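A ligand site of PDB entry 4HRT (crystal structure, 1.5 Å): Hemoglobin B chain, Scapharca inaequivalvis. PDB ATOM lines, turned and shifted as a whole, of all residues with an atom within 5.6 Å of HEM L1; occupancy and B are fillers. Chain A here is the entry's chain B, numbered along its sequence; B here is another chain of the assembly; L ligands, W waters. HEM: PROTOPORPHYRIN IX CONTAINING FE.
O1A of HEM L1 is in hydrogen-bond range of ND2 of Asn 101 of chain B (2.9 Å).
OD1 of Asn 103 lies close to O2A of HEM L1, at 3.2 Å.
An iron atom (FE) of HEM L1 is bound by a ring nitrogen (NE2) of His 104 (2.3 Å).
The side-chain amide nitrogen of Asn 101 of chain B lies within hydrogen-bond range of an oxygen (O2A) of HEM L2, 3.2 Å away.
The guanidinium group of Arg 56 lies within salt-bridge range of an oxygen (O2D) of HEM L1 (2.8 Å).
The guanidinium group (NH2) of Arg 107 lies within salt-bridge range of an oxygen (O2A) of HEM L1 (3.0 Å).
An oxygen (O1D) of HEM L1 lies within salt-bridge range of the side-chain amino group (NZ) of Lys 97 of chain B (2.7 Å).
O1A of HEM L2 lies close to OD1 of Asn 103.
Residues that only touch HEM L1: Phe 114 (3.2 Å), Phe 100 of chain A (3.2 Å), Ile 109 (3.2 Å), Lys 53 (3.3 Å), Phe 54 (3.4 Å), His 72 (3.6 Å), Leu 76 (3.6 Å), Leu 57 (3.7 Å), Ile 117 (3.8 Å), Glu 113 (3.8 Å), Ala 79 (3.8 Å), Leu 80 (3.9 Å) and Thr 75 (3.9 Å).
Water W4 bridges an oxygen (O2A) of HEM L1 (2.7 Å) and the backbone carbonyl oxygen (O) of Phe 100 of chain A (3.1 Å).
Water W1 bridges O1A of HEM L1 (2.7 Å) and NZ of Lys 97 of chain B (2.9 Å).
ND1 of His 72 sits at hydrogen-bond distance from NZ of Lys 97 of chain B, 3.0 Å away.
The backbone NH (N) of Ile 109 sits at hydrogen-bond distance from the backbone carbonyl oxygen (O) of His 104, 3.0 Å away.
A ring nitrogen (ND1) of His 104 lies within hydrogen-bond range of the backbone carbonyl oxygen (O) of Phe 100 of chain A (3.1 Å).
O of Arg 107 sits at hydrogen-bond distance from NZ of Lys 53.
The side-chain amide nitrogen (ND2) of Asn 101 of chain B sits at hydrogen-bond distance from the side-chain amide oxygen (OD1) of Asn 103 (3.3 Å).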
ATOM      1  N   LEU A  39     -29.601 -32.541   0.429  1.00  0.00           N
ATOM      2  CA  LEU A  39     -29.605 -31.264   1.152  1.00  0.00           C
ATOM      3  C   LEU A  39     -29.668 -30.106   0.160  1.00  0.00           C
ATOM      4  O   LEU A  39     -30.491 -29.205   0.323  1.00  0.00           O
ATOM      5  CB  LEU A  39     -28.361 -31.149   2.020  1.00  0.00           C
ATOM      6  CG  LEU A  39     -28.240 -29.852   2.852  1.00  0.00           C
ATOM      7  CD1 LEU A  39     -29.449 -29.663   3.751  1.00  0.00           C
ATOM      8  CD2 LEU A  39     -26.961 -29.862   3.669  1.00  0.00           C
ATOM      9  N   LEU A  43     -32.651 -27.271  -0.561  1.00  0.00           N
ATOM     10  CA  LEU A  43     -32.374 -25.832  -0.548  1.00  0.00           C
ATOM     11  C   LEU A  43     -32.930 -25.130  -1.788  1.00  0.00           C
ATOM     12  O   LEU A  43     -33.607 -24.101  -1.666  1.00  0.00           O
ATOM     13  CB  LEU A  43     -30.876 -25.554  -0.371  1.00  0.00           C
ATOM     14  CG  LEU A  43     -30.460 -24.079  -0.421  1.00  0.00           C
ATOM     15  CD1 LEU A  43     -31.025 -23.308   0.776  1.00  0.00           C
ATOM     16  CD2 LEU A  43     -28.949 -23.952  -0.485  1.00  0.00           C
ATOM     17  N   ALA A  50     -31.570 -19.067  -3.878  1.00  0.00           N
ATOM     18  CA  ALA A  50     -30.274 -19.737  -3.737  1.00  0.00           C
ATOM     19  C   ALA A  50     -29.675 -20.130  -5.093  1.00  0.00           C
ATOM     20  O   ALA A  50     -28.449 -20.173  -5.238  1.00  0.00           O
ATOM     21  CB  ALA A  50     -30.397 -20.953  -2.813  1.00  0.00           C
ATOM     22  N   LYS A  53     -27.310 -17.438  -6.220  1.00  0.00           N
ATOM     23  CA  LYS A  53     -26.022 -17.418  -5.523  1.00  0.00           C
ATOM     24  C   LYS A  53     -25.119 -18.504  -6.089  1.00  0.00           C
ATOM     25  O   LYS A  53     -23.893 -18.358  -6.136  1.00  0.00           O
ATOM     26  CB  LYS A  53     -26.200 -17.610  -4.005  1.00  0.00           C
ATOM     27  CG  LYS A  53     -26.671 -16.393  -3.239  1.00  0.00           C
ATOM     28  CD  LYS A  53     -25.646 -15.271  -3.243  1.00  0.00           C
ATOM     29  CE  LYS A  53     -26.072 -14.087  -2.392  1.00  0.00           C
ATOM     30  NZ  LYS A  53     -25.054 -13.000  -2.454  1.00  0.00           N
ATOM     31  N   PHE A  54     -25.747 -19.600  -6.523  1.00  0.00           N
ATOM     32  CA  PHE A  54     -25.037 -20.746  -7.071  1.00  0.00           C
ATOM     33  C   PHE A  54     -25.002 -20.748  -8.604  1.00  0.00           C
ATOM     34  O   PHE A  54     -24.935 -21.805  -9.228  1.00  0.00           O
ATOM     35  CB  PHE A  54     -25.667 -22.050  -6.538  1.00  0.00           C
ATOM     36  CG  PHE A  54     -25.263 -22.376  -5.121  1.00  0.00           C
ATOM     37  CD1 PHE A  54     -24.060 -23.048  -4.870  1.00  0.00           C
ATOM     38  CD2 PHE A  54     -26.073 -22.028  -4.036  1.00  0.00           C
ATOM     39  CE1 PHE A  54     -23.669 -23.364  -3.576  1.00  0.00           C
ATOM     40  CE2 PHE A  54     -25.689 -22.364  -2.727  1.00  0.00           C
ATOM     41  CZ  PHE A  54     -24.485 -23.028  -2.509  1.00  0.00           C
ATOM     42  N   ARG A  56     -22.732 -20.236 -10.794  1.00  0.00           N
ATOM     43  CA  ARG A  56     -21.605 -20.905 -11.440  1.00  0.00           C
ATOM     44  C   ARG A  56     -21.899 -22.385 -11.695  1.00  0.00           C
ATOM     45  O   ARG A  56     -21.339 -22.983 -12.625  1.00  0.00           O
ATOM     46  CB  ARG A  56     -20.324 -20.764 -10.626  1.00  0.00           C
ATOM     47  CG  ARG A  56     -19.051 -21.209 -11.354  1.00  0.00           C
ATOM     48  CD  ARG A  56     -17.892 -21.448 -10.399  1.00  0.00           C
ATOM     49  NE  ARG A  56     -18.099 -22.589  -9.520  1.00  0.00           N
ATOM     50  CZ  ARG A  56     -17.860 -23.860  -9.850  1.00  0.00           C
ATOM     51  NH1 ARG A  56     -17.393 -24.171 -11.050  1.00  0.00           N
ATOM     52  NH2 ARG A  56     -18.080 -24.818  -8.952  1.00  0.00           N
ATOM     53  N   LEU A  57     -22.786 -22.976 -10.901  1.00  0.00           N
ATOM     54  CA  LEU A  57     -23.133 -24.407 -11.052  1.00  0.00           C
ATOM     55  C   LEU A  57     -23.977 -24.692 -12.300  1.00  0.00           C
ATOM     56  O   LEU A  57     -24.145 -25.860 -12.681  1.00  0.00           O
ATOM     57  CB  LEU A  57     -23.817 -24.976  -9.796  1.00  0.00           C
ATOM     58  CG  LEU A  57     -23.115 -24.775  -8.458  1.00  0.00           C
ATOM     59  CD1 LEU A  57     -23.836 -25.549  -7.361  1.00  0.00           C
ATOM     60  CD2 LEU A  57     -21.648 -25.179  -8.504  1.00  0.00           C
ATOM     61  N   HIS A  72     -19.766 -29.779  -5.688  1.00  0.00           N
ATOM     62  CA  HIS A  72     -20.091 -28.902  -4.568  1.00  0.00           C
ATOM     63  C   HIS A  72     -20.772 -29.650  -3.402  1.00  0.00           C
ATOM     64  O   HIS A  72     -20.420 -29.456  -2.236  1.00  0.00           O
ATOM     65  CB  HIS A  72     -20.957 -27.700  -4.982  1.00  0.00           C
ATOM     66  CG  HIS A  72     -21.463 -26.959  -3.799  1.00  0.00           C
ATOM     67  ND1 HIS A  72     -20.659 -26.116  -3.058  1.00  0.00           N
ATOM     68  CD2 HIS A  72     -22.636 -27.051  -3.125  1.00  0.00           C
ATOM     69  CE1 HIS A  72     -21.343 -25.690  -2.005  1.00  0.00           C
ATOM     70  NE2 HIS A  72     -22.544 -26.243  -2.033  1.00  0.00           N
ATOM     71  N   THR A  75     -18.434 -31.830  -1.430  1.00  0.00           N
ATOM     72  CA  THR A  75     -17.496 -30.976  -0.697  1.00  0.00           C
ATOM     73  C   THR A  75     -18.144 -30.322   0.545  1.00  0.00           C
ATOM     74  O   THR A  75     -17.513 -30.246   1.601  1.00  0.00           O
ATOM     75  CB  THR A  75     -16.881 -29.941  -1.672  1.00  0.00           C
ATOM     76  OG1 THR A  75     -16.198 -30.668  -2.708  1.00  0.00           O
ATOM     77  CG2 THR A  75     -15.897 -28.989  -0.961  1.00  0.00           C
ATOM     78  N   LEU A  76     -19.416 -29.901   0.430  1.00  0.00           N
ATOM     79  CA  LEU A  76     -20.159 -29.337   1.560  1.00  0.00           C
ATOM     80  C   LEU A  76     -20.151 -30.298   2.749  1.00  0.00           C
ATOM     81  O   LEU A  76     -20.026 -29.886   3.908  1.00  0.00           O
ATOM     82  CB  LEU A  76     -21.603 -29.014   1.137  1.00  0.00           C
ATOM     83  CG  LEU A  76     -22.588 -28.500   2.184  1.00  0.00           C
ATOM     84  CD1 LEU A  76     -23.597 -27.547   1.572  1.00  0.00           C
ATOM     85  CD2 LEU A  76     -23.314 -29.616   2.917  1.00  0.00           C
ATOM     86  N   ALA A  79     -17.232 -30.103   5.097  1.00  0.00           N
ATOM     87  CA  ALA A  79     -17.235 -28.976   6.052  1.00  0.00           C
ATOM     88  C   ALA A  79     -18.069 -29.349   7.280  1.00  0.00           C
ATOM     89  O   ALA A  79     -17.682 -29.067   8.418  1.00  0.00           O
ATOM     90  CB  ALA A  79     -17.762 -27.712   5.400  1.00  0.00           C
ATOM     91  N   LEU A  80     -19.194 -30.030   7.054  1.00  0.00           N
ATOM     92  CA  LEU A  80     -19.964 -30.540   8.183  1.00  0.00           C
ATOM     93  C   LEU A  80     -19.159 -31.535   9.034  1.00  0.00           C
ATOM     94  O   LEU A  80     -19.185 -31.459  10.266  1.00  0.00           O
ATOM     95  CB  LEU A  80     -21.305 -31.141   7.740  1.00  0.00           C
ATOM     96  CG  LEU A  80     -22.315 -30.136   7.155  1.00  0.00           C
ATOM     97  CD1 LEU A  80     -23.571 -30.859   6.688  1.00  0.00           C
ATOM     98  CD2 LEU A  80     -22.664 -28.983   8.101  1.00  0.00           C
ATOM     99  N   PHE A  83     -16.844 -29.470  11.231  1.00  0.00           N
ATOM    100  CA  PHE A  83     -17.575 -28.933  12.403  1.00  0.00           C
ATOM    101  C   PHE A  83     -17.811 -30.007  13.472  1.00  0.00           C
ATOM    102  O   PHE A  83     -17.574 -29.771  14.667  1.00  0.00           O
ATOM    103  CB  PHE A  83     -18.936 -28.323  12.035  1.00  0.00           C
ATOM    104  CG  PHE A  83     -18.880 -27.162  11.061  1.00  0.00           C
ATOM    105  CD1 PHE A  83     -17.704 -26.429  10.840  1.00  0.00           C
ATOM    106  CD2 PHE A  83     -20.024 -26.789  10.371  1.00  0.00           C
ATOM    107  CE1 PHE A  83     -17.691 -25.352   9.938  1.00  0.00           C
ATOM    108  CE2 PHE A  83     -20.021 -25.722   9.473  1.00  0.00           C
ATOM    109  CZ  PHE A  83     -18.845 -25.009   9.254  1.00  0.00           C
ATOM    110  N   PHE A 100     -14.167 -21.064   7.778  1.00  0.00           N
ATOM    111  CA  PHE A 100     -15.294 -21.370   6.893  1.00  0.00           C
ATOM    112  C   PHE A 100     -16.026 -20.101   6.435  1.00  0.00           C
ATOM    113  O   PHE A 100     -16.445 -19.974   5.270  1.00  0.00           O
ATOM    114  CB  PHE A 100     -16.257 -22.308   7.625  1.00  0.00           C
ATOM    115  CG  PHE A 100     -17.566 -22.542   6.900  1.00  0.00           C
ATOM    116  CD1 PHE A 100     -18.681 -21.710   7.100  1.00  0.00           C
ATOM    117  CD2 PHE A 100     -17.703 -23.622   6.033  1.00  0.00           C
ATOM    118  CE1 PHE A 100     -19.882 -21.949   6.429  1.00  0.00           C
ATOM    119  CE2 PHE A 100     -18.899 -23.878   5.383  1.00  0.00           C
ATOM    120  CZ  PHE A 100     -19.994 -23.047   5.577  1.00  0.00           C
ATOM    121  N   ASN A 103     -14.927 -17.132   3.045  1.00  0.00           N
ATOM    122  CA  ASN A 103     -15.469 -17.115   1.674  1.00  0.00           C
ATOM    123  C   ASN A 103     -16.955 -16.770   1.616  1.00  0.00           C
ATOM    124  O   ASN A 103     -17.427 -16.165   0.642  1.00  0.00           O
ATOM    125  CB  ASN A 103     -15.275 -18.469   0.967  1.00  0.00           C
ATOM    126  CG  ASN A 103     -13.811 -18.813   0.687  1.00  0.00           C
ATOM    127  OD1 ASN A 103     -13.467 -19.987   0.537  1.00  0.00           O
ATOM    128  ND2 ASN A 103     -12.949 -17.807   0.625  1.00  0.00           N
ATOM    129  N   HIS A 104     -17.710 -17.159   2.646  1.00  0.00           N
ATOM    130  CA  HIS A 104     -19.155 -16.898   2.667  1.00  0.00           C
ATOM    131  C   HIS A 104     -19.448 -15.397   2.868  1.00  0.00           C
ATOM    132  O   HIS A 104     -20.339 -14.848   2.216  1.00  0.00           O
ATOM    133  CB  HIS A 104     -19.868 -17.799   3.690  1.00  0.00           C
ATOM    134  CG  HIS A 104     -19.952 -19.242   3.257  1.00  0.00           C
ATOM    135  ND1 HIS A 104     -18.927 -20.141   3.443  1.00  0.00           N
ATOM    136  CD2 HIS A 104     -20.920 -19.899   2.588  1.00  0.00           C
ATOM    137  CE1 HIS A 104     -19.279 -21.313   2.926  1.00  0.00           C
ATOM    138  NE2 HIS A 104     -20.484 -21.187   2.401  1.00  0.00           N
ATOM    139  N   ARG A 107     -18.751 -13.722  -0.472  1.00  0.00           N
ATOM    140  CA  ARG A 107     -19.828 -13.915  -1.443  1.00  0.00           C
ATOM    141  C   ARG A 107     -21.115 -13.198  -1.038  1.00  0.00           C
ATOM    142  O   ARG A 107     -22.137 -13.304  -1.709  1.00  0.00           O
ATOM    143  CB  ARG A 107     -20.103 -15.413  -1.671  1.00  0.00           C
ATOM    144  CG  ARG A 107     -19.106 -16.096  -2.591  1.00  0.00           C
ATOM    145  CD  ARG A 107     -19.487 -17.535  -2.826  1.00  0.00           C
ATOM    146  NE  ARG A 107     -19.411 -18.291  -1.591  1.00  0.00           N
ATOM    147  CZ  ARG A 107     -18.413 -19.117  -1.247  1.00  0.00           C
ATOM    148  NH1 ARG A 107     -17.392 -19.300  -2.073  1.00  0.00           N
ATOM    149  NH2 ARG A 107     -18.457 -19.748  -0.074  1.00  0.00           N
ATOM    150  N   ILE A 109     -23.065 -13.626   1.618  1.00  0.00           N
ATOM    151  CA  ILE A 109     -24.098 -14.467   2.204  1.00  0.00           C
ATOM    152  C   ILE A 109     -24.293 -14.052   3.662  1.00  0.00           C
ATOM    153  O   ILE A 109     -23.453 -14.322   4.522  1.00  0.00           O
ATOM    154  CB  ILE A 109     -23.727 -15.959   2.095  1.00  0.00           C
ATOM    155  CG1 ILE A 109     -23.503 -16.325   0.625  1.00  0.00           C
ATOM    156  CG2 ILE A 109     -24.815 -16.838   2.711  1.00  0.00           C
ATOM    157  CD1 ILE A 109     -22.588 -17.499   0.438  1.00  0.00           C
ATOM    158  N   GLU A 113     -29.528 -15.218   5.175  1.00  0.00           N
ATOM    159  CA  GLU A 113     -29.499 -16.101   4.003  1.00  0.00           C
ATOM    160  C   GLU A 113     -28.951 -17.491   4.368  1.00  0.00           C
ATOM    161  O   GLU A 113     -29.476 -18.507   3.928  1.00  0.00           O
ATOM    162  CB  GLU A 113     -28.720 -15.495   2.822  1.00  0.00           C
ATOM    163  CG  GLU A 113     -28.813 -16.328   1.545  1.00  0.00           C
ATOM    164  CD  GLU A 113     -28.243 -15.646   0.321  1.00  0.00           C
ATOM    165  OE1 GLU A 113     -27.399 -14.724   0.460  1.00  0.00           O
ATOM    166  OE2 GLU A 113     -28.629 -16.028  -0.808  1.00  0.00           O
ATOM    167  N   PHE A 114     -27.900 -17.532   5.189  1.00  0.00           N
ATOM    168  CA  PHE A 114     -27.287 -18.810   5.557  1.00  0.00           C
ATOM    169  C   PHE A 114     -28.286 -19.707   6.305  1.00  0.00           C
ATOM    170  O   PHE A 114     -28.297 -20.928   6.114  1.00  0.00           O
ATOM    171  CB  PHE A 114     -26.027 -18.587   6.401  1.00  0.00           C
ATOM    172  CG  PHE A 114     -25.167 -19.813   6.537  1.00  0.00           C
ATOM    173  CD1 PHE A 114     -24.213 -20.141   5.555  1.00  0.00           C
ATOM    174  CD2 PHE A 114     -25.297 -20.653   7.639  1.00  0.00           C
ATOM    175  CE1 PHE A 114     -23.414 -21.268   5.690  1.00  0.00           C
ATOM    176  CE2 PHE A 114     -24.510 -21.790   7.767  1.00  0.00           C
ATOM    177  CZ  PHE A 114     -23.550 -22.096   6.803  1.00  0.00           C
ATOM    178  N   GLY A 115     -29.132 -19.090   7.137  1.00  0.00           N
ATOM    179  CA  GLY A 115     -30.171 -19.817   7.881  1.00  0.00           C
ATOM    180  C   GLY A 115     -31.225 -20.502   7.020  1.00  0.00           C
ATOM    181  O   GLY A 115     -32.008 -21.317   7.533  1.00  0.00           O
ATOM    182  N   GLU A 116     -31.252 -20.192   5.728  1.00  0.00           N
ATOM    183  CA  GLU A 116     -32.066 -20.945   4.763  1.00  0.00           C
ATOM    184  C   GLU A 116     -31.726 -22.441   4.726  1.00  0.00           C
ATOM    185  O   GLU A 116     -32.500 -23.245   4.203  1.00  0.00           O
ATOM    186  CB  GLU A 116     -31.944 -20.373   3.353  1.00  0.00           C
ATOM    187  CG  GLU A 116     -32.557 -18.989   3.164  1.00  0.00           C
ATOM    188  CD  GLU A 116     -32.198 -18.379   1.819  1.00  0.00           C
ATOM    189  OE1 GLU A 116     -31.449 -19.022   1.049  1.00  0.00           O
ATOM    190  OE2 GLU A 116     -32.657 -17.264   1.527  1.00  0.00           O
ATOM    191  N   ILE A 117     -30.565 -22.817   5.255  1.00  0.00           N
ATOM    192  CA  ILE A 117     -30.165 -24.230   5.246  1.00  0.00           C
ATOM    193  C   ILE A 117     -30.905 -25.070   6.281  1.00  0.00           C
ATOM    194  O   ILE A 117     -30.947 -26.298   6.130  1.00  0.00           O
ATOM    195  CB  ILE A 117     -28.624 -24.387   5.376  1.00  0.00           C
ATOM    196  CG1 ILE A 117     -28.124 -25.712   4.757  1.00  0.00           C
ATOM    197  CG2 ILE A 117     -28.173 -24.239   6.821  1.00  0.00           C
ATOM    198  CD1 ILE A 117     -28.269 -25.813   3.253  1.00  0.00           C
ATOM    199  N   VAL A 145     -25.672 -24.309  13.452  1.00  0.00           N
ATOM    200  CA  VAL A 145     -25.774 -23.319  12.370  1.00  0.00           C
ATOM    201  C   VAL A 145     -25.733 -21.877  12.909  1.00  0.00           C
ATOM    202  O   VAL A 145     -25.114 -21.022  12.293  1.00  0.00           O
ATOM    203  CB  VAL A 145     -27.034 -23.576  11.488  1.00  0.00           C
ATOM    204  CG1 VAL A 145     -27.349 -22.381  10.595  1.00  0.00           C
ATOM    205  CG2 VAL A 145     -26.849 -24.850  10.672  1.00  0.00           C
ATOM    206  N   LYS B  97     -13.948 -28.642  -8.521  1.00  0.00           N
ATOM    207  CA  LYS B  97     -14.579 -27.796  -7.489  1.00  0.00           C
ATOM    208  C   LYS B  97     -13.512 -27.110  -6.621  1.00  0.00           C
ATOM    209  O   LYS B  97     -13.537 -25.887  -6.410  1.00  0.00           O
ATOM    210  CB  LYS B  97     -15.540 -28.631  -6.611  1.00  0.00           C
ATOM    211  CG  LYS B  97     -15.963 -28.007  -5.274  1.00  0.00           C
ATOM    212  CD  LYS B  97     -16.848 -26.782  -5.424  1.00  0.00           C
ATOM    213  CE  LYS B  97     -17.231 -26.225  -4.051  1.00  0.00           C
ATOM    214  NZ  LYS B  97     -18.041 -24.973  -4.120  1.00  0.00           N
ATOM    215  N   VAL B 100     -11.481 -24.083  -8.143  1.00  0.00           N
ATOM    216  CA  VAL B 100     -12.129 -22.787  -8.418  1.00  0.00           C
ATOM    217  C   VAL B 100     -11.528 -21.638  -7.605  1.00  0.00           C
ATOM    218  O   VAL B 100     -11.102 -20.621  -8.181  1.00  0.00           O
ATOM    219  CB  VAL B 100     -13.669 -22.834  -8.239  1.00  0.00           C
ATOM    220  CG1 VAL B 100     -14.288 -21.465  -8.487  1.00  0.00           C
ATOM    221  CG2 VAL B 100     -14.307 -23.855  -9.188  1.00  0.00           C
ATOM    222  N   ASN B 101     -11.477 -21.784  -6.272  1.00  0.00           N
ATOM    223  CA  ASN B 101     -10.936 -20.685  -5.448  1.00  0.00           C
ATOM    224  C   ASN B 101      -9.433 -20.507  -5.618  1.00  0.00           C
ATOM    225  O   ASN B 101      -8.920 -19.397  -5.486  1.00  0.00           O
ATOM    226  CB  ASN B 101     -11.236 -20.880  -3.958  1.00  0.00           C
ATOM    227  CG  ASN B 101     -12.709 -20.802  -3.621  1.00  0.00           C
ATOM    228  OD1 ASN B 101     -13.523 -20.241  -4.369  1.00  0.00           O
ATOM    229  ND2 ASN B 101     -13.069 -21.348  -2.469  1.00  0.00           N
HETATM  230  CHA HEM L   1     -19.141 -22.877  -1.251  1.00  0.00           C
HETATM  231  CHB HEM L   1     -20.047 -25.385   2.796  1.00  0.00           C
HETATM  232  CHC HEM L   1     -24.330 -23.035   3.206  1.00  0.00           C
HETATM  233  CHD HEM L   1     -23.287 -20.406  -0.733  1.00  0.00           C
HETATM  234  C1A HEM L   1     -18.972 -23.725  -0.159  1.00  0.00           C
HETATM  235  C2A HEM L   1     -17.847 -24.581   0.046  1.00  0.00           C
HETATM  236  C3A HEM L   1     -18.107 -25.307   1.196  1.00  0.00           C
HETATM  237  C4A HEM L   1     -19.390 -24.885   1.668  1.00  0.00           C
HETATM  238  CMA HEM L   1     -17.207 -26.356   1.869  1.00  0.00           C
HETATM  239  CAA HEM L   1     -16.586 -24.663  -0.783  1.00  0.00           C
HETATM  240  CBA HEM L   1     -15.484 -23.805  -0.128  1.00  0.00           C
HETATM  241  CGA HEM L   1     -15.818 -22.339  -0.331  1.00  0.00           C
HETATM  242  O1A HEM L   1     -15.761 -21.846  -1.486  1.00  0.00           O
HETATM  243  O2A HEM L   1     -16.178 -21.626   0.637  1.00  0.00           O
HETATM  244  C1B HEM L   1     -21.344 -25.007   3.223  1.00  0.00           C
HETATM  245  C2B HEM L   1     -22.055 -25.621   4.313  1.00  0.00           C
HETATM  246  C3B HEM L   1     -23.256 -24.968   4.439  1.00  0.00           C
HETATM  247  C4B HEM L   1     -23.269 -23.936   3.371  1.00  0.00           C
HETATM  248  CMB HEM L   1     -21.552 -26.748   5.168  1.00  0.00           C
HETATM  249  CAB HEM L   1     -24.373 -25.196   5.391  1.00  0.00           C
HETATM  250  CBB HEM L   1     -24.598 -26.337   6.025  1.00  0.00           C
HETATM  251  C1C HEM L   1     -24.432 -22.102   2.161  1.00  0.00           C
HETATM  252  C2C HEM L   1     -25.604 -21.377   1.834  1.00  0.00           C
HETATM  253  C3C HEM L   1     -25.298 -20.619   0.700  1.00  0.00           C
HETATM  254  C4C HEM L   1     -23.931 -20.908   0.369  1.00  0.00           C
HETATM  255  CMC HEM L   1     -26.905 -21.411   2.602  1.00  0.00           C
HETATM  256  CAC HEM L   1     -26.135 -19.649  -0.077  1.00  0.00           C
HETATM  257  CBC HEM L   1     -27.464 -19.566  -0.042  1.00  0.00           C
HETATM  258  C1D HEM L   1     -22.103 -20.980  -1.216  1.00  0.00           C
HETATM  259  C2D HEM L   1     -21.580 -20.610  -2.555  1.00  0.00           C
HETATM  260  C3D HEM L   1     -20.431 -21.297  -2.715  1.00  0.00           C
HETATM  261  C4D HEM L   1     -20.284 -22.090  -1.445  1.00  0.00           C
HETATM  262  CMD HEM L   1     -22.218 -19.646  -3.544  1.00  0.00           C
HETATM  263  CAD HEM L   1     -19.535 -21.297  -3.960  1.00  0.00           C
HETATM  264  CBD HEM L   1     -20.200 -22.320  -4.933  1.00  0.00           C
HETATM  265  CGD HEM L   1     -19.457 -22.626  -6.222  1.00  0.00           C
HETATM  266  O1D HEM L   1     -18.915 -23.752  -6.411  1.00  0.00           O
HETATM  267  O2D HEM L   1     -19.392 -21.772  -7.150  1.00  0.00           O
HETATM  268  NA  HEM L   1     -19.861 -23.841   0.895  1.00  0.00           N
HETATM  269  NB  HEM L   1     -22.034 -23.934   2.813  1.00  0.00           N
HETATM  270  NC  HEM L   1     -23.403 -21.767   1.297  1.00  0.00           N
HETATM  271  ND  HEM L   1     -21.227 -21.774  -0.497  1.00  0.00           N
HETATM  272 FE   HEM L   1     -21.588 -22.772   1.123  1.00  0.00          FE
HETATM  273  CHA HEM L   2      -7.489 -22.207   1.012  1.00  0.00           C
HETATM  274  CHB HEM L   2      -6.772 -26.979   0.439  1.00  0.00           C
HETATM  275  CHC HEM L   2      -2.342 -26.059  -1.408  1.00  0.00           C
HETATM  276  CHD HEM L   2      -3.226 -21.308  -1.171  1.00  0.00           C
HETATM  277  C1A HEM L   2      -7.713 -23.589   0.958  1.00  0.00           C
HETATM  278  C2A HEM L   2      -8.874 -24.238   1.449  1.00  0.00           C
HETATM  279  C3A HEM L   2      -8.668 -25.594   1.302  1.00  0.00           C
HETATM  280  C4A HEM L   2      -7.385 -25.746   0.702  1.00  0.00           C
HETATM  281  CMA HEM L   2      -9.636 -26.726   1.656  1.00  0.00           C
HETATM  282  CAA HEM L   2     -10.149 -23.607   2.015  1.00  0.00           C
HETATM  283  CBA HEM L   2     -11.234 -23.459   0.922  1.00  0.00           C
HETATM  284  CGA HEM L   2     -10.838 -22.420  -0.096  1.00  0.00           C
HETATM  285  O1A HEM L   2     -10.889 -21.210   0.208  1.00  0.00           O
HETATM  286  O2A HEM L   2     -10.481 -22.737  -1.243  1.00  0.00           O
HETATM  287  C1B HEM L   2      -5.454 -27.140  -0.035  1.00  0.00           C
HETATM  288  C2B HEM L   2      -4.801 -28.423  -0.189  1.00  0.00           C
HETATM  289  C3B HEM L   2      -3.547 -28.165  -0.692  1.00  0.00           C
HETATM  290  C4B HEM L   2      -3.468 -26.684  -0.867  1.00  0.00           C
HETATM  291  CMB HEM L   2      -5.385 -29.771   0.179  1.00  0.00           C
HETATM  292  CAB HEM L   2      -2.434 -29.090  -1.040  1.00  0.00           C
HETATM  293  CBB HEM L   2      -2.224 -30.248  -0.413  1.00  0.00           C
HETATM  294  C1C HEM L   2      -2.194 -24.675  -1.552  1.00  0.00           C
HETATM  295  C2C HEM L   2      -0.999 -24.038  -1.957  1.00  0.00           C
HETATM  296  C3C HEM L   2      -1.252 -22.650  -1.904  1.00  0.00           C
HETATM  297  C4C HEM L   2      -2.607 -22.512  -1.449  1.00  0.00           C
HETATM  298  CMC HEM L   2       0.273 -24.737  -2.380  1.00  0.00           C
HETATM  299  CAC HEM L   2      -0.351 -21.518  -2.238  1.00  0.00           C
HETATM  300  CBC HEM L   2       0.674 -21.604  -3.095  1.00  0.00           C
HETATM  301  C1D HEM L   2      -4.423 -21.225  -0.444  1.00  0.00           C
HETATM  302  C2D HEM L   2      -4.896 -19.908   0.085  1.00  0.00           C
HETATM  303  C3D HEM L   2      -6.083 -20.157   0.683  1.00  0.00           C
HETATM  304  C4D HEM L   2      -6.305 -21.627   0.532  1.00  0.00           C
HETATM  305  CMD HEM L   2      -4.202 -18.581  -0.073  1.00  0.00           C
HETATM  306  CAD HEM L   2      -6.961 -19.167   1.418  1.00  0.00           C
HETATM  307  CBD HEM L   2      -6.296 -19.001   2.810  1.00  0.00           C
HETATM  308  CGD HEM L   2      -7.006 -18.144   3.854  1.00  0.00           C
HETATM  309  O1D HEM L   2      -6.954 -16.905   3.781  1.00  0.00           O
HETATM  310  O2D HEM L   2      -7.624 -18.637   4.823  1.00  0.00           O
HETATM  311  NA  HEM L   2      -6.827 -24.510   0.434  1.00  0.00           N
HETATM  312  NB  HEM L   2      -4.687 -26.167  -0.578  1.00  0.00           N
HETATM  313  NC  HEM L   2      -3.170 -23.756  -1.273  1.00  0.00           N
HETATM  314  ND  HEM L   2      -5.343 -22.230  -0.261  1.00  0.00           N
HETATM  315 FE   HEM L   2      -5.046 -24.132  -0.458  1.00  0.00          FE
HETATM  316  O   HOH W   1     -15.908 -23.059  -3.892  1.00  0.00           O
HETATM  317  O   HOH W   2     -18.703 -19.051  -7.555  1.00  0.00           O
HETATM  318  O   HOH W   3     -22.075 -16.491  -4.918  1.00  0.00           O
HETATM  319  O   HOH W   4     -15.561 -22.104   3.185  1.00  0.00           O
